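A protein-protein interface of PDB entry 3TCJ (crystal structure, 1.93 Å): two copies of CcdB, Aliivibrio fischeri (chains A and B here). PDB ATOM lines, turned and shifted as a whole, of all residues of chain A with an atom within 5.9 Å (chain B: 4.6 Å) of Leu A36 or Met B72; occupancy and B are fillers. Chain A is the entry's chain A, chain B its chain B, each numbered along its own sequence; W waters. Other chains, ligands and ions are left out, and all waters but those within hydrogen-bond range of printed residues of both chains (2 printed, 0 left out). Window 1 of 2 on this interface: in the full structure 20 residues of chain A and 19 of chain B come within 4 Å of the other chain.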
ATOM      1  N   VAL A  22     -13.244  19.195  -1.370  1.00  0.00           N
ATOM      2  CA  VAL A  22     -13.309  17.872  -1.972  1.00  0.00           C
ATOM      3  C   VAL A  22     -14.686  17.239  -1.781  1.00  0.00           C
ATOM      4  O   VAL A  22     -15.247  17.260  -0.687  1.00  0.00           O
ATOM      5  CB  VAL A  22     -12.217  16.938  -1.401  1.00  0.00           C
ATOM      6  CG1 VAL A  22     -12.331  16.849   0.111  1.00  0.00           C
ATOM      7  CG2 VAL A  22     -12.313  15.558  -2.031  1.00  0.00           C
ATOM      8  N   ASP A  23     -15.229  16.689  -2.862  1.00  0.00           N
ATOM      9  CA  ASP A  23     -16.506  15.988  -2.821  1.00  0.00           C
ATOM     10  C   ASP A  23     -16.309  14.634  -2.147  1.00  0.00           C
ATOM     11  O   ASP A  23     -15.513  13.821  -2.606  1.00  0.00           O
ATOM     12  CB  ASP A  23     -17.029  15.800  -4.245  1.00  0.00           C
ATOM     13  CG  ASP A  23     -18.406  15.170  -4.292  1.00  0.00           C
ATOM     14  OD1 ASP A  23     -18.947  14.798  -3.228  1.00  0.00           O
ATOM     15  OD2 ASP A  23     -18.949  15.050  -5.411  1.00  0.00           O
ATOM     16  N   VAL A  24     -17.022  14.393  -1.051  1.00  0.00           N
ATOM     17  CA  VAL A  24     -16.874  13.138  -0.321  1.00  0.00           C
ATOM     18  C   VAL A  24     -18.143  12.294  -0.376  1.00  0.00           C
ATOM     19  O   VAL A  24     -18.265  11.290   0.324  1.00  0.00           O
ATOM     20  CB  VAL A  24     -16.468  13.379   1.148  1.00  0.00           C
ATOM     21  CG1 VAL A  24     -15.094  14.031   1.216  1.00  0.00           C
ATOM     22  CG2 VAL A  24     -17.512  14.228   1.859  1.00  0.00           C
ATOM     23  N   GLN A  25     -19.082  12.704  -1.222  1.00  0.00           N
ATOM     24  CA  GLN A  25     -20.366  12.026  -1.340  1.00  0.00           C
ATOM     25  C   GLN A  25     -20.300  10.869  -2.334  1.00  0.00           C
ATOM     26  O   GLN A  25     -19.668  10.976  -3.386  1.00  0.00           O
ATOM     27  CB  GLN A  25     -21.448  13.023  -1.755  1.00  0.00           C
ATOM     28  CG  GLN A  25     -22.849  12.446  -1.837  1.00  0.00           C
ATOM     29  CD  GLN A  25     -23.905  13.529  -1.920  1.00  0.00           C
ATOM     30  OE1 GLN A  25     -24.035  14.353  -1.016  1.00  0.00           O
ATOM     31  NE2 GLN A  25     -24.667  13.534  -3.009  1.00  0.00           N
ATOM     32  N   THR A  34     -27.367  18.330  -4.175  1.00  0.00           N
ATOM     33  CA  THR A  34     -26.431  18.805  -3.164  1.00  0.00           C
ATOM     34  C   THR A  34     -25.281  17.818  -3.015  1.00  0.00           C
ATOM     35  O   THR A  34     -25.404  16.648  -3.381  1.00  0.00           O
ATOM     36  CB  THR A  34     -27.106  19.004  -1.792  1.00  0.00           C
ATOM     37  OG1 THR A  34     -27.675  17.765  -1.350  1.00  0.00           O
ATOM     38  CG2 THR A  34     -28.194  20.063  -1.879  1.00  0.00           C
ATOM     39  N   ARG A  35     -24.166  18.299  -2.479  1.00  0.00           N
ATOM     40  CA  ARG A  35     -22.989  17.472  -2.268  1.00  0.00           C
ATOM     41  C   ARG A  35     -22.412  17.700  -0.881  1.00  0.00           C
ATOM     42  O   ARG A  35     -22.268  18.840  -0.439  1.00  0.00           O
ATOM     43  CB  ARG A  35     -21.917  17.788  -3.317  1.00  0.00           C
ATOM     44  CG  ARG A  35     -22.296  17.414  -4.741  1.00  0.00           C
ATOM     45  CD  ARG A  35     -22.242  15.908  -4.955  1.00  0.00           C
ATOM     46  NE  ARG A  35     -22.514  15.554  -6.346  1.00  0.00           N
ATOM     47  CZ  ARG A  35     -23.732  15.368  -6.842  1.00  0.00           C
ATOM     48  NH1 ARG A  35     -24.794  15.499  -6.059  1.00  0.00           N
ATOM     49  NH2 ARG A  35     -23.889  15.051  -8.120  1.00  0.00           N
ATOM     50  N   LEU A  36     -22.089  16.612  -0.197  1.00  0.00           N
ATOM     51  CA  LEU A  36     -21.327  16.707   1.034  1.00  0.00           C
ATOM     52  C   LEU A  36     -19.870  16.946   0.655  1.00  0.00           C
ATOM     53  O   LEU A  36     -19.266  16.141  -0.053  1.00  0.00           O
ATOM     54  CB  LEU A  36     -21.461  15.420   1.847  1.00  0.00           C
ATOM     55  CG  LEU A  36     -20.949  15.484   3.286  1.00  0.00           C
ATOM     56  CD1 LEU A  36     -21.787  16.450   4.115  1.00  0.00           C
ATOM     57  CD2 LEU A  36     -20.954  14.097   3.902  1.00  0.00           C
ATOM     58  N   VAL A  37     -19.311  18.066   1.102  1.00  0.00           N
ATOM     59  CA  VAL A  37     -17.937  18.407   0.758  1.00  0.00           C
ATOM     60  C   VAL A  37     -17.134  18.827   1.979  1.00  0.00           C
ATOM     61  O   VAL A  37     -17.695  19.206   3.005  1.00  0.00           O
ATOM     62  CB  VAL A  37     -17.876  19.541  -0.286  1.00  0.00           C
ATOM     63  CG1 VAL A  37     -18.705  19.187  -1.513  1.00  0.00           C
ATOM     64  CG2 VAL A  37     -18.342  20.856   0.327  1.00  0.00           C
ATOM     65  N   ILE A  38     -15.814  18.758   1.854  1.00  0.00           N
ATOM     66  CA  ILE A  38     -14.912  19.173   2.917  1.00  0.00           C
ATOM     67  C   ILE A  38     -13.902  20.170   2.372  1.00  0.00           C
ATOM     68  O   ILE A  38     -13.228  19.893   1.378  1.00  0.00           O
ATOM     69  CB  ILE A  38     -14.154  17.975   3.505  1.00  0.00           C
ATOM     70  CG1 ILE A  38     -15.138  16.915   4.006  1.00  0.00           C
ATOM     71  CG2 ILE A  38     -13.232  18.430   4.623  1.00  0.00           C
ATOM     72  CD1 ILE A  38     -14.470  15.657   4.513  1.00  0.00           C
ATOM     73  N   MET A  72     -17.040  19.801   7.337  1.00  0.00           N
ATOM     74  CA  MET A  72     -17.770  19.137   6.270  1.00  0.00           C
ATOM     75  C   MET A  72     -19.189  19.687   6.228  1.00  0.00           C
ATOM     76  O   MET A  72     -19.833  19.838   7.266  1.00  0.00           O
ATOM     77  CB  MET A  72     -17.795  17.631   6.524  1.00  0.00           C
ATOM     78  CG  MET A  72     -18.558  16.819   5.498  1.00  0.00           C
ATOM     79  SD  MET A  72     -18.467  15.052   5.849  1.00  0.00           S
ATOM     80  N   THR A  73     -19.675  19.992   5.031  1.00  0.00           N
ATOM     81  CA  THR A  73     -20.999  20.581   4.893  1.00  0.00           C
ATOM     82  C   THR A  73     -21.664  20.209   3.572  1.00  0.00           C
ATOM     83  O   THR A  73     -20.995  19.851   2.604  1.00  0.00           O
ATOM     84  CB  THR A  73     -20.937  22.116   5.002  1.00  0.00           C
ATOM     85  OG1 THR A  73     -22.264  22.650   5.069  1.00  0.00           O
ATOM     86  CG2 THR A  73     -20.211  22.706   3.801  1.00  0.00           C
ATOM     87  N   SER A  74     -22.989  20.293   3.548  1.00  0.00           N
ATOM     88  CA  SER A  74     -23.755  20.060   2.331  1.00  0.00           C
ATOM     89  C   SER A  74     -23.881  21.355   1.537  1.00  0.00           C
ATOM     90  O   SER A  74     -24.338  22.370   2.061  1.00  0.00           O
ATOM     91  CB  SER A  74     -25.141  19.516   2.674  1.00  0.00           C
ATOM     92  OG  SER A  74     -25.987  19.539   1.537  1.00  0.00           O
ATOM     93  N   VAL A  75     -23.472  21.316   0.274  1.00  0.00           N
ATOM     94  CA  VAL A  75     -23.535  22.491  -0.586  1.00  0.00           C
ATOM     95  C   VAL A  75     -24.290  22.178  -1.872  1.00  0.00           C
ATOM     96  O   VAL A  75     -24.360  21.023  -2.288  1.00  0.00           O
ATOM     97  CB  VAL A  75     -22.126  22.993  -0.956  1.00  0.00           C
ATOM     98  CG1 VAL A  75     -21.340  23.362   0.300  1.00  0.00           C
ATOM     99  CG2 VAL A  75     -21.387  21.943  -1.778  1.00  0.00           C
ATOM    100  N   ILE A  98     -13.570  11.161   8.333  1.00  0.00           N
ATOM    101  CA  ILE A  98     -14.996  11.347   8.563  1.00  0.00           C
ATOM    102  C   ILE A  98     -15.499  10.383   9.635  1.00  0.00           C
ATOM    103  O   ILE A  98     -16.242  10.772  10.539  1.00  0.00           O
ATOM    104  CB  ILE A  98     -15.797  11.127   7.270  1.00  0.00           C
ATOM    105  CG1 ILE A  98     -15.381  12.152   6.205  1.00  0.00           C
ATOM    106  CG2 ILE A  98     -17.282  11.222   7.552  1.00  0.00           C
ATOM    107  CD1 ILE A  98     -15.928  11.861   4.820  1.00  0.00           C
ATOM    108  N   VAL B  24     -24.254  14.867  15.690  1.00  0.00           N
ATOM    109  CA  VAL B  24     -23.766  13.538  15.335  1.00  0.00           C
ATOM    110  C   VAL B  24     -22.255  13.420  15.509  1.00  0.00           C
ATOM    111  O   VAL B  24     -21.653  12.421  15.118  1.00  0.00           O
ATOM    112  CB  VAL B  24     -24.142  13.162  13.888  1.00  0.00           C
ATOM    113  CG1 VAL B  24     -25.656  13.011  13.753  1.00  0.00           C
ATOM    114  CG2 VAL B  24     -23.603  14.198  12.909  1.00  0.00           C
ATOM    115  N   LEU B  36     -20.873  18.853  13.969  1.00  0.00           N
ATOM    116  CA  LEU B  36     -21.550  18.275  12.818  1.00  0.00           C
ATOM    117  C   LEU B  36     -22.967  17.887  13.225  1.00  0.00           C
ATOM    118  O   LEU B  36     -23.157  17.100  14.150  1.00  0.00           O
ATOM    119  CB  LEU B  36     -20.793  17.044  12.321  1.00  0.00           C
ATOM    120  CG  LEU B  36     -21.315  16.370  11.053  1.00  0.00           C
ATOM    121  CD1 LEU B  36     -21.191  17.305   9.861  1.00  0.00           C
ATOM    122  CD2 LEU B  36     -20.556  15.075  10.806  1.00  0.00           C
ATOM    123  N   VAL B  37     -23.962  18.451  12.547  1.00  0.00           N
ATOM    124  CA  VAL B  37     -25.353  18.195  12.903  1.00  0.00           C
ATOM    125  C   VAL B  37     -26.202  17.836  11.688  1.00  0.00           C
ATOM    126  O   VAL B  37     -25.845  18.147  10.552  1.00  0.00           O
ATOM    127  CB  VAL B  37     -25.990  19.405  13.629  1.00  0.00           C
ATOM    128  CG1 VAL B  37     -25.166  19.792  14.850  1.00  0.00           C
ATOM    129  CG2 VAL B  37     -26.128  20.586  12.681  1.00  0.00           C
ATOM    130  N   ILE B  38     -27.328  17.175  11.939  1.00  0.00           N
ATOM    131  CA  ILE B  38     -28.270  16.827  10.882  1.00  0.00           C
ATOM    132  C   ILE B  38     -29.673  17.298  11.260  1.00  0.00           C
ATOM    133  O   ILE B  38     -30.162  16.993  12.347  1.00  0.00           O
ATOM    134  CB  ILE B  38     -28.288  15.310  10.617  1.00  0.00           C
ATOM    135  CG1 ILE B  38     -26.862  14.776  10.453  1.00  0.00           C
ATOM    136  CG2 ILE B  38     -29.121  14.993   9.383  1.00  0.00           C
ATOM    137  CD1 ILE B  38     -26.801  13.290  10.163  1.00  0.00           C
ATOM    138  N   PRO B  39     -30.325  18.048  10.360  1.00  0.00           N
ATOM    139  CA  PRO B  39     -31.634  18.637  10.662  1.00  0.00           C
ATOM    140  C   PRO B  39     -32.783  17.639  10.532  1.00  0.00           C
ATOM    141  O   PRO B  39     -32.689  16.670   9.776  1.00  0.00           O
ATOM    142  CB  PRO B  39     -31.769  19.735   9.604  1.00  0.00           C
ATOM    143  CG  PRO B  39     -30.944  19.267   8.459  1.00  0.00           C
ATOM    144  CD  PRO B  39     -29.852  18.389   9.006  1.00  0.00           C
ATOM    145  N   LEU B  68     -32.856  14.601   7.446  1.00  0.00           N
ATOM    146  CA  LEU B  68     -32.320  14.958   6.137  1.00  0.00           C
ATOM    147  C   LEU B  68     -30.796  14.897   6.121  1.00  0.00           C
ATOM    148  O   LEU B  68     -30.121  15.924   6.181  1.00  0.00           O
ATOM    149  CB  LEU B  68     -32.810  16.346   5.716  1.00  0.00           C
ATOM    150  CG  LEU B  68     -34.307  16.440   5.410  1.00  0.00           C
ATOM    151  CD1 LEU B  68     -34.699  17.862   5.042  1.00  0.00           C
ATOM    152  CD2 LEU B  68     -34.694  15.472   4.301  1.00  0.00           C
ATOM    153  N   THR B  69     -30.267  13.682   6.034  1.00  0.00           N
ATOM    154  CA  THR B  69     -28.827  13.452   6.053  1.00  0.00           C
ATOM    155  C   THR B  69     -28.106  14.252   4.973  1.00  0.00           C
ATOM    156  O   THR B  69     -26.971  14.690   5.164  1.00  0.00           O
ATOM    157  CB  THR B  69     -28.508  11.957   5.864  1.00  0.00           C
ATOM    158  OG1 THR B  69     -29.381  11.176   6.688  1.00  0.00           O
ATOM    159  CG2 THR B  69     -27.060  11.662   6.232  1.00  0.00           C
ATOM    160  N   GLN B  70     -28.772  14.444   3.839  1.00  0.00           N
ATOM    161  CA  GLN B  70     -28.180  15.163   2.716  1.00  0.00           C
ATOM    162  C   GLN B  70     -28.004  16.651   3.024  1.00  0.00           C
ATOM    163  O   GLN B  70     -27.367  17.378   2.265  1.00  0.00           O
ATOM    164  CB  GLN B  70     -29.030  14.977   1.455  1.00  0.00           C
ATOM    165  CG  GLN B  70     -30.366  15.699   1.490  1.00  0.00           C
ATOM    166  CD  GLN B  70     -31.359  15.138   0.489  1.00  0.00           C
ATOM    167  OE1 GLN B  70     -31.778  13.983   0.593  1.00  0.00           O
ATOM    168  NE2 GLN B  70     -31.745  15.954  -0.486  1.00  0.00           N
ATOM    169  N   GLN B  71     -28.571  17.096   4.141  1.00  0.00           N
ATOM    170  CA  GLN B  71     -28.443  18.486   4.568  1.00  0.00           C
ATOM    171  C   GLN B  71     -27.536  18.607   5.791  1.00  0.00           C
ATOM    172  O   GLN B  71     -27.541  19.625   6.484  1.00  0.00           O
ATOM    173  CB  GLN B  71     -29.820  19.085   4.865  1.00  0.00           C
ATOM    174  CG  GLN B  71     -30.630  19.422   3.624  1.00  0.00           C
ATOM    175  CD  GLN B  71     -30.086  20.629   2.884  1.00  0.00           C
ATOM    176  OE1 GLN B  71     -29.850  21.683   3.478  1.00  0.00           O
ATOM    177  NE2 GLN B  71     -29.887  20.484   1.579  1.00  0.00           N
ATOM    178  N   MET B  72     -26.764  17.556   6.053  1.00  0.00           N
ATOM    179  CA  MET B  72     -25.825  17.552   7.168  1.00  0.00           C
ATOM    180  C   MET B  72     -24.837  18.702   7.014  1.00  0.00           C
ATOM    181  O   MET B  72     -24.397  19.003   5.904  1.00  0.00           O
ATOM    182  CB  MET B  72     -25.080  16.217   7.220  1.00  0.00           C
ATOM    183  CG  MET B  72     -24.174  16.045   8.424  1.00  0.00           C
ATOM    184  SD  MET B  72     -23.520  14.368   8.540  1.00  0.00           S
ATOM    185  CE  MET B  72     -22.700  14.223   6.954  1.00  0.00           C
ATOM    186  N   THR B  73     -24.491  19.351   8.121  1.00  0.00           N
ATOM    187  CA  THR B  73     -23.595  20.500   8.058  1.00  0.00           C
ATOM    188  C   THR B  73     -22.886  20.787   9.376  1.00  0.00           C
ATOM    189  O   THR B  73     -23.370  20.432  10.450  1.00  0.00           O
ATOM    190  CB  THR B  73     -24.347  21.775   7.622  1.00  0.00           C
ATOM    191  OG1 THR B  73     -23.416  22.854   7.470  1.00  0.00           O
ATOM    192  CG2 THR B  73     -25.394  22.155   8.655  1.00  0.00           C
ATOM    193  N   ILE B  98     -25.338   8.111   7.405  1.00  0.00           N
ATOM    194  CA  ILE B  98     -24.101   8.788   7.039  1.00  0.00           C
ATOM    195  C   ILE B  98     -23.188   7.834   6.267  1.00  0.00           C
ATOM    196  O   ILE B  98     -22.603   8.206   5.250  1.00  0.00           O
ATOM    197  CB  ILE B  98     -23.367   9.338   8.281  1.00  0.00           C
ATOM    198  CG1 ILE B  98     -24.250  10.349   9.016  1.00  0.00           C
ATOM    199  CG2 ILE B  98     -22.048   9.973   7.882  1.00  0.00           C
ATOM    200  CD1 ILE B  98     -23.590  10.978  10.227  1.00  0.00           C
ATOM    201  N   LEU B 101     -24.492   7.749   2.856  1.00  0.00           N
ATOM    202  CA  LEU B 101     -24.192   8.987   2.145  1.00  0.00           C
ATOM    203  C   LEU B 101     -22.779   8.964   1.569  1.00  0.00           C
ATOM    204  O   LEU B 101     -22.518   9.534   0.510  1.00  0.00           O
ATOM    205  CB  LEU B 101     -24.357  10.186   3.081  1.00  0.00           C
ATOM    206  CG  LEU B 101     -24.164  11.580   2.482  1.00  0.00           C
ATOM    207  CD1 LEU B 101     -25.248  11.885   1.462  1.00  0.00           C
ATOM    208  CD2 LEU B 101     -24.149  12.633   3.581  1.00  0.00           C
ATOM    209  N   ILE B 102     -21.874   8.284   2.267  1.00  0.00           N
ATOM    210  CA  ILE B 102     -20.460   8.314   1.915  1.00  0.00           C
ATOM    211  C   ILE B 102     -19.972   7.069   1.169  1.00  0.00           C
ATOM    212  O   ILE B 102     -19.018   7.141   0.395  1.00  0.00           O
ATOM    213  CB  ILE B 102     -19.586   8.522   3.170  1.00  0.00           C
ATOM    214  CG1 ILE B 102     -20.015   9.790   3.906  1.00  0.00           C
ATOM    215  CG2 ILE B 102     -18.123   8.609   2.791  1.00  0.00           C
ATOM    216  CD1 ILE B 102     -19.941  11.030   3.056  1.00  0.00           C
HETATM  217  O   HOH W   1     -30.250  18.265  -0.576  1.00  0.00           O
HETATM  218  O   HOH W   2     -25.850  16.155  -0.161  1.00  0.00           O
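Leu A36 touches three residues of chain B. Of chain A, only Leu A36 (3.5 Å), Thr A73 (3.8 Å) and Ser A74 (3.0 Å) come within 4 Å of Met B72. Of the printed residues of chain B, Met A72 touches Leu B36 and Thr B73. Of the printed residues of chain A, Gln B71 touches Thr A34 (3.9 Å) and Ser A74 (3.9 Å). Of the printed residues of chain B, Thr A73 touches Met B72 and Thr B73. Asp A23 touches none of the printed residues of chain B. The nearest printed residue of chain B that does not touch Leu A36 is Thr B69 (5.6 Å).
Water W2 lies within hydrogen-bond range of OE1 of Gln A25, OG1 of Thr A34 and O of Gln B70. Water W1 lies within hydrogen-bond range of the side-chain hydroxyl (OG1) of Thr A34 (2.7 Å), the side-chain amide nitrogen (NE2) of Gln B70 (2.8 Å) and the side-chain amide nitrogen (NE2) of Gln B71 (3.1 Å).
Hydrophobic or aromatic side chains of chain B that line the printed part of chain A: Leu B36, Met B72, Leu B101 and Ile B102. Along chain B the printed residues that touch a printed residue of chain A span positions 36 to 102. Among the printed residues, 14 pairs touch across the chains.
Among the printed residues, pairs that only touch across the chains: Val A24 with Ile B102, Leu A36 with Ile B102, Leu A36 with Met B72, Leu A36 with Leu B101, Thr A34 with Gln B70, Gln A25 with Leu B101, Thr A73 with Met B72, Met A72 with Thr B73, Met A72 with Leu B36, Thr A34 with Gln B71 and Ser A74 with Gln B71.
Leu A36 touches Met B72, and with the chains exchanged Met A72 touches Leu B36. Met A72 touches Thr B73, and with the chains exchanged Thr A73 touches Met B72. Thr B73 touches its own counterpart, Thr A73. Of the 14 pairs that touch across the chains among the printed residues, 5 have their exchanged pair printed and touching as well.
The side-chain hydroxyl of Thr A73 lies within hydrogen-bond range of the side-chain hydroxyl of Thr B73. O of Gln B70 lies within hydrogen-bond range of OG of Ser A74, 2.7 Å away. The backbone NH of Ser A74 sits at hydrogen-bond distance from the backbone carbonyl oxygen of Met B72 (3.0 Å).
The side-chain amide nitrogen (NE2) of Gln A25 lies within hydrogen-bond range of the backbone carbonyl oxygen (O) of Thr A34, at 3.2 Å. The backbone carbonyl oxygen (O) of Leu A36 lies within hydrogen-bond range of the backbone NH (N) of Val A24. The backbone NH (N) of Val B37 is in hydrogen-bond range of the backbone carbonyl oxygen (O) of Thr B73. The backbone carbonyl oxygen (O) of Thr A73 is in hydrogen-bond range of the backbone NH (N) of Val A37 (2.9 Å). The side-chain amide oxygen of Gln A25 lies within hydrogen-bond range of the backbone NH of Leu A36. OD1 of Asp A23 is in hydrogen-bond range of N of Gln A25.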
